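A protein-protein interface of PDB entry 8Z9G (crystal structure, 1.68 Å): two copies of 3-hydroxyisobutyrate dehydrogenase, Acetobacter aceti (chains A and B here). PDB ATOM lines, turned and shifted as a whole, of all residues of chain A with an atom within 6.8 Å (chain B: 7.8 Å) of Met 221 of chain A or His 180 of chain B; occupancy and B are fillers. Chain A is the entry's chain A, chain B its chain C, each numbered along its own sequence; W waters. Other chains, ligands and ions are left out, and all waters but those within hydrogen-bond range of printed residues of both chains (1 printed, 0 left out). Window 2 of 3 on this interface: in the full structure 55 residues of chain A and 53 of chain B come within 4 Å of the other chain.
Of the printed residues of chain B, Met 221 of chain A touches His 180 (3.96 Å) and Ala 181 (3.2 Å).
Of the printed residues of chain B, Ala 225 of chain A touches Ile 179.
Gly 158 of chain B touches none of the printed residues of chain A.
Asp 160 of chain B touches none of the printed residues of chain A.
Of the printed residues of chain A, Ile 179 of chain B touches Ala 225 (3.9 Å).
Of the printed residues of chain A, His 180 of chain B touches Met 221.
Of the printed residues of chain A, Ser 186 of chain B touches Leu 217.
Of the printed residues of chain A, Leu 190 of chain B touches Leu 217 and Leu 222.
The nearest printed residue of chain B that does not touch Ala 225 of chain A is Leu 190 of chain B (4.1 Å).
Among the printed residues, merely in contact across the chains: Leu 217 of chain A with Ser 186 of chain B, Leu 217 of chain A with Leu 190 of chain B, Met 221 of chain A with His 180 of chain B, Met 221 of chain A with Ala 181 of chain B, Leu 222 of chain A with Leu 190 of chain B and Ala 225 of chain A with Ile 179 of chain B.
The backbone NH of Val 157 of chain B is in hydrogen-bond range of the backbone carbonyl oxygen of Ile 179 of chain B (3.0 Å).
The backbone carbonyl oxygen of Gly 159 of chain B sits at hydrogen-bond distance from a ring nitrogen (NE2) of His 180 of chain B.
The side-chain carboxylate (OD1) of Asp 218 of chain A sits at hydrogen-bond distance from the backbone NH (N) of Met 221 of chain A.
The backbone carbonyl oxygen of Ile 155 of chain B lies within hydrogen-bond range of the backbone NH of Ile 179 of chain B.
O of Val 157 of chain B sits at hydrogen-bond distance from N of Ala 181 of chain B (2.8 Å).
O of Gly 182 of chain B lies within hydrogen-bond range of NE2 of His 180 of chain B (3.2 Å).
No position is printed for both chains.
Of the 6 pairs that touch across the chains among the printed residues, none has its exchanged pair printed and touching as well.
Water W1 bridges the backbone carbonyl oxygen (O) of Ala 181 of chain B and the backbone NH (N) of Asp 218 of chain A.
Of the 24 printed residues of chain B, 5 touch a printed residue of chain A.
Along chain B the printed residues that touch a printed residue of chain A span positions 179 to 190.
Printed residues of chain A that touch a printed residue of chain B: Leu 217, Met 221, Leu 222 and Ala 225.
Hydrophobic or aromatic side chains of chain A within 4 Å of the printed part of chain B: Leu 217, Met 221, Leu 222 and Ala 225.
Among the printed residues, 6 pairs touch across the chains.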
ATOM      1  N   LEU A 217     -12.197  26.340 -22.412  1.00  0.00           N
ATOM      2  CA  LEU A 217     -13.583  25.951 -22.615  1.00  0.00           C
ATOM      3  C   LEU A 217     -14.243  25.693 -21.267  1.00  0.00           C
ATOM      4  O   LEU A 217     -13.643  25.087 -20.374  1.00  0.00           O
ATOM      5  CB  LEU A 217     -13.668  24.700 -23.499  1.00  0.00           C
ATOM      6  CG  LEU A 217     -13.217  24.850 -24.969  1.00  0.00           C
ATOM      7  CD1 LEU A 217     -13.399  23.530 -25.726  1.00  0.00           C
ATOM      8  CD2 LEU A 217     -13.993  25.944 -25.648  1.00  0.00           C
ATOM      9  N   ASP A 218     -15.482  26.165 -21.131  1.00  0.00           N
ATOM     10  CA  ASP A 218     -16.268  25.949 -19.917  1.00  0.00           C
ATOM     11  C   ASP A 218     -16.430  24.458 -19.652  1.00  0.00           C
ATOM     12  O   ASP A 218     -16.777  23.697 -20.557  1.00  0.00           O
ATOM     13  CB  ASP A 218     -17.636  26.627 -20.092  1.00  0.00           C
ATOM     14  CG  ASP A 218     -18.553  26.455 -18.901  1.00  0.00           C
ATOM     15  OD1 ASP A 218     -19.142  25.360 -18.745  1.00  0.00           O
ATOM     16  OD2 ASP A 218     -18.729  27.443 -18.145  1.00  0.00           O
ATOM     17  N   ARG A 219     -16.164  24.033 -18.407  1.00  0.00           N
ATOM     18  CA  ARG A 219     -16.155  22.602 -18.095  1.00  0.00           C
ATOM     19  C   ARG A 219     -17.522  21.972 -18.315  1.00  0.00           C
ATOM     20  O   ARG A 219     -17.639  20.885 -18.893  1.00  0.00           O
ATOM     21  CB  ARG A 219     -15.710  22.369 -16.655  1.00  0.00           C
ATOM     22  CG  ARG A 219     -15.589  20.866 -16.306  1.00  0.00           C
ATOM     23  CD  ARG A 219     -15.489  20.668 -14.808  1.00  0.00           C
ATOM     24  NE  ARG A 219     -15.147  19.295 -14.450  1.00  0.00           N
ATOM     25  CZ  ARG A 219     -16.007  18.396 -13.993  1.00  0.00           C
ATOM     26  NH1 ARG A 219     -17.288  18.686 -13.824  1.00  0.00           N
ATOM     27  NH2 ARG A 219     -15.570  17.175 -13.691  1.00  0.00           N
ATOM     28  N   SER A 220     -18.575  22.620 -17.824  1.00  0.00           N
ATOM     29  CA  SER A 220     -19.900  22.032 -17.964  1.00  0.00           C
ATOM     30  C   SER A 220     -20.328  21.972 -19.427  1.00  0.00           C
ATOM     31  O   SER A 220     -20.919  20.976 -19.862  1.00  0.00           O
ATOM     32  CB  SER A 220     -20.906  22.836 -17.142  1.00  0.00           C
ATOM     33  OG  SER A 220     -20.541  22.803 -15.769  1.00  0.00           O
ATOM     34  N   MET A 221     -20.042  23.028 -20.189  1.00  0.00           N
ATOM     35  CA  MET A 221     -20.374  23.046 -21.608  1.00  0.00           C
ATOM     36  C   MET A 221     -19.673  21.898 -22.316  1.00  0.00           C
ATOM     37  O   MET A 221     -20.296  21.138 -23.063  1.00  0.00           O
ATOM     38  CB  MET A 221     -19.932  24.380 -22.203  1.00  0.00           C
ATOM     39  CG  MET A 221     -20.044  24.621 -23.712  1.00  0.00           C
ATOM     40  SD  MET A 221     -19.110  23.599 -24.880  1.00  0.00           S
ATOM     41  CE  MET A 221     -17.488  24.308 -24.740  1.00  0.00           C
ATOM     42  N   LEU A 222     -18.367  21.764 -22.073  1.00  0.00           N
ATOM     43  CA  LEU A 222     -17.542  20.775 -22.778  1.00  0.00           C
ATOM     44  C   LEU A 222     -17.986  19.339 -22.494  1.00  0.00           C
ATOM     45  O   LEU A 222     -18.092  18.521 -23.415  1.00  0.00           O
ATOM     46  CB  LEU A 222     -16.075  20.978 -22.387  1.00  0.00           C
ATOM     47  CG  LEU A 222     -15.060  19.949 -22.900  1.00  0.00           C
ATOM     48  CD1 LEU A 222     -15.071  19.934 -24.427  1.00  0.00           C
ATOM     49  CD2 LEU A 222     -13.664  20.283 -22.362  1.00  0.00           C
ATOM     50  N   PHE A 223     -18.218  18.993 -21.220  1.00  0.00           N
ATOM     51  CA  PHE A 223     -18.677  17.645 -20.914  1.00  0.00           C
ATOM     52  C   PHE A 223     -20.009  17.359 -21.597  1.00  0.00           C
ATOM     53  O   PHE A 223     -20.206  16.275 -22.160  1.00  0.00           O
ATOM     54  CB  PHE A 223     -18.807  17.444 -19.402  1.00  0.00           C
ATOM     55  CG  PHE A 223     -17.523  17.053 -18.718  1.00  0.00           C
ATOM     56  CD1 PHE A 223     -16.493  17.966 -18.559  1.00  0.00           C
ATOM     57  CD2 PHE A 223     -17.367  15.761 -18.209  1.00  0.00           C
ATOM     58  CE1 PHE A 223     -15.318  17.613 -17.910  1.00  0.00           C
ATOM     59  CE2 PHE A 223     -16.192  15.393 -17.562  1.00  0.00           C
ATOM     60  CZ  PHE A 223     -15.170  16.320 -17.403  1.00  0.00           C
ATOM     61  N   ASP A 224     -20.932  18.329 -21.565  1.00  0.00           N
ATOM     62  CA  ASP A 224     -22.245  18.108 -22.164  1.00  0.00           C
ATOM     63  C   ASP A 224     -22.161  18.020 -23.684  1.00  0.00           C
ATOM     64  O   ASP A 224     -22.897  17.240 -24.308  1.00  0.00           O
ATOM     65  CB  ASP A 224     -23.199  19.228 -21.769  1.00  0.00           C
ATOM     66  CG  ASP A 224     -23.719  19.075 -20.351  1.00  0.00           C
ATOM     67  OD1 ASP A 224     -23.384  18.079 -19.677  1.00  0.00           O
ATOM     68  OD2 ASP A 224     -24.493  19.951 -19.929  1.00  0.00           O
ATOM     69  N   ALA A 225     -21.291  18.831 -24.288  1.00  0.00           N
ATOM     70  CA  ALA A 225     -21.145  18.822 -25.742  1.00  0.00           C
ATOM     71  C   ALA A 225     -20.633  17.478 -26.221  1.00  0.00           C
ATOM     72  O   ALA A 225     -21.094  16.945 -27.233  1.00  0.00           O
ATOM     73  CB  ALA A 225     -20.193  19.927 -26.185  1.00  0.00           C
ATOM     74  N   LEU A 226     -19.665  16.913 -25.509  1.00  0.00           N
ATOM     75  CA  LEU A 226     -19.112  15.649 -25.976  1.00  0.00           C
ATOM     76  C   LEU A 226     -20.124  14.513 -25.884  1.00  0.00           C
ATOM     77  O   LEU A 226     -20.022  13.538 -26.632  1.00  0.00           O
ATOM     78  CB  LEU A 226     -17.837  15.347 -25.198  1.00  0.00           C
ATOM     79  CG  LEU A 226     -16.722  16.345 -25.504  1.00  0.00           C
ATOM     80  CD1 LEU A 226     -15.494  16.034 -24.645  1.00  0.00           C
ATOM     81  CD2 LEU A 226     -16.338  16.356 -26.988  1.00  0.00           C
ATOM     82  N   LYS A 244     -18.103  13.919 -14.944  1.00  0.00           N
ATOM     83  CA  LYS A 244     -18.628  15.263 -14.703  1.00  0.00           C
ATOM     84  C   LYS A 244     -19.054  15.416 -13.250  1.00  0.00           C
ATOM     85  O   LYS A 244     -18.859  16.483 -12.642  1.00  0.00           O
ATOM     86  CB  LYS A 244     -19.808  15.553 -15.631  1.00  0.00           C
ATOM     87  CG  LYS A 244     -20.228  17.036 -15.677  1.00  0.00           C
ATOM     88  CD  LYS A 244     -21.553  17.184 -16.404  1.00  0.00           C
ATOM     89  CE  LYS A 244     -21.997  18.661 -16.461  1.00  0.00           C
ATOM     90  NZ  LYS A 244     -23.425  18.784 -16.921  1.00  0.00           N
ATOM     91  N   LEU B 137     -17.723  34.383 -37.028  1.00  0.00           N
ATOM     92  CA  LEU B 137     -18.064  33.234 -36.196  1.00  0.00           C
ATOM     93  C   LEU B 137     -17.138  32.084 -36.559  1.00  0.00           C
ATOM     94  O   LEU B 137     -16.987  31.770 -37.748  1.00  0.00           O
ATOM     95  CB  LEU B 137     -19.510  32.802 -36.436  1.00  0.00           C
ATOM     96  CG  LEU B 137     -20.611  33.778 -36.020  1.00  0.00           C
ATOM     97  CD1 LEU B 137     -21.968  33.126 -36.205  1.00  0.00           C
ATOM     98  CD2 LEU B 137     -20.398  34.175 -34.577  1.00  0.00           C
ATOM     99  N   ILE B 155     -22.905  21.694 -35.304  1.00  0.00           N
ATOM    100  CA  ILE B 155     -22.172  22.941 -35.466  1.00  0.00           C
ATOM    101  C   ILE B 155     -21.557  23.294 -34.118  1.00  0.00           C
ATOM    102  O   ILE B 155     -22.239  23.258 -33.092  1.00  0.00           O
ATOM    103  CB  ILE B 155     -23.086  24.076 -35.970  1.00  0.00           C
ATOM    104  CG1 ILE B 155     -23.431  23.949 -37.468  1.00  0.00           C
ATOM    105  CG2 ILE B 155     -22.401  25.406 -35.785  1.00  0.00           C
ATOM    106  CD1 ILE B 155     -23.981  22.624 -37.930  1.00  0.00           C
ATOM    107  N   LEU B 156     -20.270  23.616 -34.119  1.00  0.00           N
ATOM    108  CA  LEU B 156     -19.515  23.978 -32.915  1.00  0.00           C
ATOM    109  C   LEU B 156     -19.119  25.443 -33.057  1.00  0.00           C
ATOM    110  O   LEU B 156     -18.161  25.758 -33.768  1.00  0.00           O
ATOM    111  CB  LEU B 156     -18.282  23.084 -32.782  1.00  0.00           C
ATOM    112  CG  LEU B 156     -18.485  21.609 -33.159  1.00  0.00           C
ATOM    113  CD1 LEU B 156     -17.150  20.891 -33.327  1.00  0.00           C
ATOM    114  CD2 LEU B 156     -19.335  20.912 -32.105  1.00  0.00           C
ATOM    115  N   VAL B 157     -19.839  26.365 -32.408  1.00  0.00           N
ATOM    116  CA  VAL B 157     -19.697  27.768 -32.788  1.00  0.00           C
ATOM    117  C   VAL B 157     -19.211  28.624 -31.622  1.00  0.00           C
ATOM    118  O   VAL B 157     -19.665  28.469 -30.483  1.00  0.00           O
ATOM    119  CB  VAL B 157     -21.004  28.347 -33.378  1.00  0.00           C
ATOM    120  CG1 VAL B 157     -22.139  28.323 -32.371  1.00  0.00           C
ATOM    121  CG2 VAL B 157     -20.751  29.759 -33.918  1.00  0.00           C
ATOM    122  N   GLY B 158     -18.280  29.523 -31.921  1.00  0.00           N
ATOM    123  CA  GLY B 158     -17.778  30.502 -30.964  1.00  0.00           C
ATOM    124  C   GLY B 158     -18.203  31.907 -31.361  1.00  0.00           C
ATOM    125  O   GLY B 158     -18.120  32.280 -32.534  1.00  0.00           O
ATOM    126  N   GLY B 159     -18.666  32.671 -30.390  1.00  0.00           N
ATOM    127  CA  GLY B 159     -19.041  34.049 -30.642  1.00  0.00           C
ATOM    128  C   GLY B 159     -20.094  34.518 -29.657  1.00  0.00           C
ATOM    129  O   GLY B 159     -20.522  33.789 -28.764  1.00  0.00           O
ATOM    130  N   ASP B 160     -20.503  35.771 -29.846  1.00  0.00           N
ATOM    131  CA  ASP B 160     -21.557  36.355 -29.029  1.00  0.00           C
ATOM    132  C   ASP B 160     -22.884  35.688 -29.357  1.00  0.00           C
ATOM    133  O   ASP B 160     -23.194  35.429 -30.523  1.00  0.00           O
ATOM    134  CB  ASP B 160     -21.639  37.869 -29.271  1.00  0.00           C
ATOM    135  CG  ASP B 160     -22.515  38.602 -28.247  1.00  0.00           C
ATOM    136  OD1 ASP B 160     -23.620  38.119 -27.916  1.00  0.00           O
ATOM    137  OD2 ASP B 160     -22.092  39.684 -27.779  1.00  0.00           O
ATOM    138  N   LYS B 161     -23.676  35.427 -28.313  1.00  0.00           N
ATOM    139  CA  LYS B 161     -24.945  34.725 -28.474  1.00  0.00           C
ATOM    140  C   LYS B 161     -25.862  35.421 -29.478  1.00  0.00           C
ATOM    141  O   LYS B 161     -26.619  34.750 -30.190  1.00  0.00           O
ATOM    142  CB  LYS B 161     -25.610  34.577 -27.098  1.00  0.00           C
ATOM    143  CG  LYS B 161     -27.063  35.014 -26.982  1.00  0.00           C
ATOM    144  CD  LYS B 161     -27.596  34.714 -25.571  1.00  0.00           C
ATOM    145  CE  LYS B 161     -29.105  34.903 -25.470  1.00  0.00           C
ATOM    146  NZ  LYS B 161     -29.610  34.662 -24.077  1.00  0.00           N
ATOM    147  N   ASP B 162     -25.770  36.749 -29.589  1.00  0.00           N
ATOM    148  CA  ASP B 162     -26.621  37.479 -30.529  1.00  0.00           C
ATOM    149  C   ASP B 162     -26.178  37.249 -31.970  1.00  0.00           C
ATOM    150  O   ASP B 162     -27.013  37.204 -32.883  1.00  0.00           O
ATOM    151  CB  ASP B 162     -26.602  38.973 -30.205  1.00  0.00           C
ATOM    152  CG  ASP B 162     -27.573  39.340 -29.095  1.00  0.00           C
ATOM    153  OD1 ASP B 162     -28.360  38.467 -28.662  1.00  0.00           O
ATOM    154  OD2 ASP B 162     -27.550  40.509 -28.661  1.00  0.00           O
ATOM    155  N   ASP B 163     -24.866  37.111 -32.198  1.00  0.00           N
ATOM    156  CA  ASP B 163     -24.375  36.833 -33.546  1.00  0.00           C
ATOM    157  C   ASP B 163     -24.646  35.388 -33.949  1.00  0.00           C
ATOM    158  O   ASP B 163     -24.889  35.107 -35.131  1.00  0.00           O
ATOM    159  CB  ASP B 163     -22.881  37.149 -33.631  1.00  0.00           C
ATOM    160  CG  ASP B 163     -22.593  38.634 -33.482  1.00  0.00           C
ATOM    161  OD1 ASP B 163     -23.373  39.447 -34.019  1.00  0.00           O
ATOM    162  OD2 ASP B 163     -21.597  38.995 -32.821  1.00  0.00           O
ATOM    163  N   VAL B 164     -24.608  34.462 -32.987  1.00  0.00           N
ATOM    164  CA  VAL B 164     -24.997  33.080 -33.257  1.00  0.00           C
ATOM    165  C   VAL B 164     -26.462  33.016 -33.671  1.00  0.00           C
ATOM    166  O   VAL B 164     -26.830  32.287 -34.601  1.00  0.00           O
ATOM    167  CB  VAL B 164     -24.714  32.197 -32.025  1.00  0.00           C
ATOM    168  CG1 VAL B 164     -25.239  30.796 -32.242  1.00  0.00           C
ATOM    169  CG2 VAL B 164     -23.227  32.161 -31.733  1.00  0.00           C
ATOM    170  N   ALA B 165     -27.317  33.786 -32.990  1.00  0.00           N
ATOM    171  CA  ALA B 165     -28.736  33.828 -33.332  1.00  0.00           C
ATOM    172  C   ALA B 165     -28.955  34.288 -34.770  1.00  0.00           C
ATOM    173  O   ALA B 165     -29.837  33.770 -35.466  1.00  0.00           O
ATOM    174  CB  ALA B 165     -29.474  34.751 -32.365  1.00  0.00           C
ATOM    175  N   LEU B 177     -27.986  20.249 -34.998  1.00  0.00           N
ATOM    176  CA  LEU B 177     -27.699  20.712 -33.648  1.00  0.00           C
ATOM    177  C   LEU B 177     -26.597  21.757 -33.697  1.00  0.00           C
ATOM    178  O   LEU B 177     -25.572  21.548 -34.355  1.00  0.00           O
ATOM    179  CB  LEU B 177     -27.273  19.549 -32.753  1.00  0.00           C
ATOM    180  CG  LEU B 177     -26.859  19.935 -31.328  1.00  0.00           C
ATOM    181  CD1 LEU B 177     -28.028  20.527 -30.583  1.00  0.00           C
ATOM    182  CD2 LEU B 177     -26.275  18.733 -30.573  1.00  0.00           C
ATOM    183  N   THR B 178     -26.798  22.875 -33.006  1.00  0.00           N
ATOM    184  CA  THR B 178     -25.819  23.954 -32.910  1.00  0.00           C
ATOM    185  C   THR B 178     -25.389  24.050 -31.455  1.00  0.00           C
ATOM    186  O   THR B 178     -26.202  24.390 -30.590  1.00  0.00           O
ATOM    187  CB  THR B 178     -26.403  25.286 -33.394  1.00  0.00           C
ATOM    188  OG1 THR B 178     -26.709  25.204 -34.793  1.00  0.00           O
ATOM    189  CG2 THR B 178     -25.418  26.432 -33.153  1.00  0.00           C
ATOM    190  N   ILE B 179     -24.126  23.733 -31.182  1.00  0.00           N
ATOM    191  CA  ILE B 179     -23.564  23.837 -29.841  1.00  0.00           C
ATOM    192  C   ILE B 179     -22.845  25.176 -29.749  1.00  0.00           C
ATOM    193  O   ILE B 179     -21.870  25.419 -30.468  1.00  0.00           O
ATOM    194  CB  ILE B 179     -22.621  22.667 -29.525  1.00  0.00           C
ATOM    195  CG1 ILE B 179     -23.367  21.337 -29.651  1.00  0.00           C
ATOM    196  CG2 ILE B 179     -21.978  22.858 -28.142  1.00  0.00           C
ATOM    197  CD1 ILE B 179     -22.524  20.107 -29.339  1.00  0.00           C
ATOM    198  N   HIS B 180     -23.340  26.063 -28.889  1.00  0.00           N
ATOM    199  CA  HIS B 180     -22.674  27.335 -28.632  1.00  0.00           C
ATOM    200  C   HIS B 180     -21.561  27.100 -27.621  1.00  0.00           C
ATOM    201  O   HIS B 180     -21.827  26.887 -26.433  1.00  0.00           O
ATOM    202  CB  HIS B 180     -23.665  28.375 -28.119  1.00  0.00           C
ATOM    203  CG  HIS B 180     -23.070  29.738 -27.979  1.00  0.00           C
ATOM    204  ND1 HIS B 180     -23.667  30.743 -27.245  1.00  0.00           N
ATOM    205  CD2 HIS B 180     -21.919  30.260 -28.463  1.00  0.00           C
ATOM    206  CE1 HIS B 180     -22.915  31.829 -27.298  1.00  0.00           C
ATOM    207  NE2 HIS B 180     -21.846  31.561 -28.027  1.00  0.00           N
ATOM    208  N   ALA B 181     -20.314  27.136 -28.079  1.00  0.00           N
ATOM    209  CA  ALA B 181     -19.216  26.642 -27.257  1.00  0.00           C
ATOM    210  C   ALA B 181     -18.603  27.709 -26.369  1.00  0.00           C
ATOM    211  O   ALA B 181     -17.757  27.387 -25.526  1.00  0.00           O
ATOM    212  CB  ALA B 181     -18.125  26.032 -28.154  1.00  0.00           C
ATOM    213  N   GLY B 182     -19.007  28.960 -26.524  1.00  0.00           N
ATOM    214  CA  GLY B 182     -18.370  30.052 -25.832  1.00  0.00           C
ATOM    215  C   GLY B 182     -18.128  31.227 -26.753  1.00  0.00           C
ATOM    216  O   GLY B 182     -18.689  31.309 -27.851  1.00  0.00           O
ATOM    217  N   PRO B 183     -17.275  32.167 -26.321  1.00  0.00           N
ATOM    218  CA  PRO B 183     -16.959  33.331 -27.165  1.00  0.00           C
ATOM    219  C   PRO B 183     -16.052  32.972 -28.329  1.00  0.00           C
ATOM    220  O   PRO B 183     -15.708  31.797 -28.488  1.00  0.00           O
ATOM    221  CB  PRO B 183     -16.263  34.301 -26.201  1.00  0.00           C
ATOM    222  CG  PRO B 183     -15.860  33.506 -25.026  1.00  0.00           C
ATOM    223  CD  PRO B 183     -16.740  32.290 -24.952  1.00  0.00           C
ATOM    224  N   THR B 184     -15.650  33.968 -29.126  1.00  0.00           N
ATOM    225  CA  THR B 184     -14.823  33.706 -30.301  1.00  0.00           C
ATOM    226  C   THR B 184     -13.622  32.845 -29.935  1.00  0.00           C
ATOM    227  O   THR B 184     -12.974  33.060 -28.907  1.00  0.00           O
ATOM    228  CB  THR B 184     -14.330  35.014 -30.936  1.00  0.00           C
ATOM    229  OG1 THR B 184     -13.347  34.703 -31.935  1.00  0.00           O
ATOM    230  CG2 THR B 184     -13.692  35.921 -29.904  1.00  0.00           C
ATOM    231  N   SER B 186     -13.956  29.592 -29.324  1.00  0.00           N
ATOM    232  CA  SER B 186     -14.409  28.399 -28.619  1.00  0.00           C
ATOM    233  C   SER B 186     -14.809  27.281 -29.569  1.00  0.00           C
ATOM    234  O   SER B 186     -14.644  26.105 -29.236  1.00  0.00           O
ATOM    235  CB  SER B 186     -15.570  28.751 -27.698  1.00  0.00           C
ATOM    236  OG  SER B 186     -15.170  29.791 -26.835  1.00  0.00           O
ATOM    237  N   GLY B 187     -15.349  27.613 -30.743  1.00  0.00           N
ATOM    238  CA  GLY B 187     -15.703  26.560 -31.680  1.00  0.00           C
ATOM    239  C   GLY B 187     -14.474  25.882 -32.248  1.00  0.00           C
ATOM    240  O   GLY B 187     -14.415  24.648 -32.333  1.00  0.00           O
ATOM    241  N   ARG B 189     -11.631  25.584 -30.789  1.00  0.00           N
ATOM    242  CA  ARG B 189     -11.067  24.725 -29.747  1.00  0.00           C
ATOM    243  C   ARG B 189     -11.876  23.445 -29.568  1.00  0.00           C
ATOM    244  O   ARG B 189     -11.301  22.362 -29.439  1.00  0.00           O
ATOM    245  CB  ARG B 189     -10.982  25.493 -28.431  1.00  0.00           C
ATOM    246  CG  ARG B 189      -9.876  26.533 -28.403  1.00  0.00           C
ATOM    247  CD  ARG B 189     -10.210  27.657 -27.422  1.00  0.00           C
ATOM    248  NE  ARG B 189      -9.067  28.532 -27.200  1.00  0.00           N
ATOM    249  CZ  ARG B 189      -8.653  29.457 -28.053  1.00  0.00           C
ATOM    250  NH1 ARG B 189      -9.275  29.664 -29.205  1.00  0.00           N
ATOM    251  NH2 ARG B 189      -7.591  30.195 -27.747  1.00  0.00           N
ATOM    252  N   LEU B 190     -13.207  23.546 -29.550  1.00  0.00           N
ATOM    253  CA  LEU B 190     -14.029  22.351 -29.392  1.00  0.00           C
ATOM    254  C   LEU B 190     -13.834  21.387 -30.559  1.00  0.00           C
ATOM    255  O   LEU B 190     -13.846  20.165 -30.368  1.00  0.00           O
ATOM    256  CB  LEU B 190     -15.505  22.748 -29.241  1.00  0.00           C
ATOM    257  CG  LEU B 190     -16.509  21.617 -28.983  1.00  0.00           C
ATOM    258  CD1 LEU B 190     -16.080  20.700 -27.837  1.00  0.00           C
ATOM    259  CD2 LEU B 190     -17.897  22.197 -28.700  1.00  0.00           C
HETATM  260  O   HOH W   1     -16.620  28.070 -23.156  1.00  0.00           O
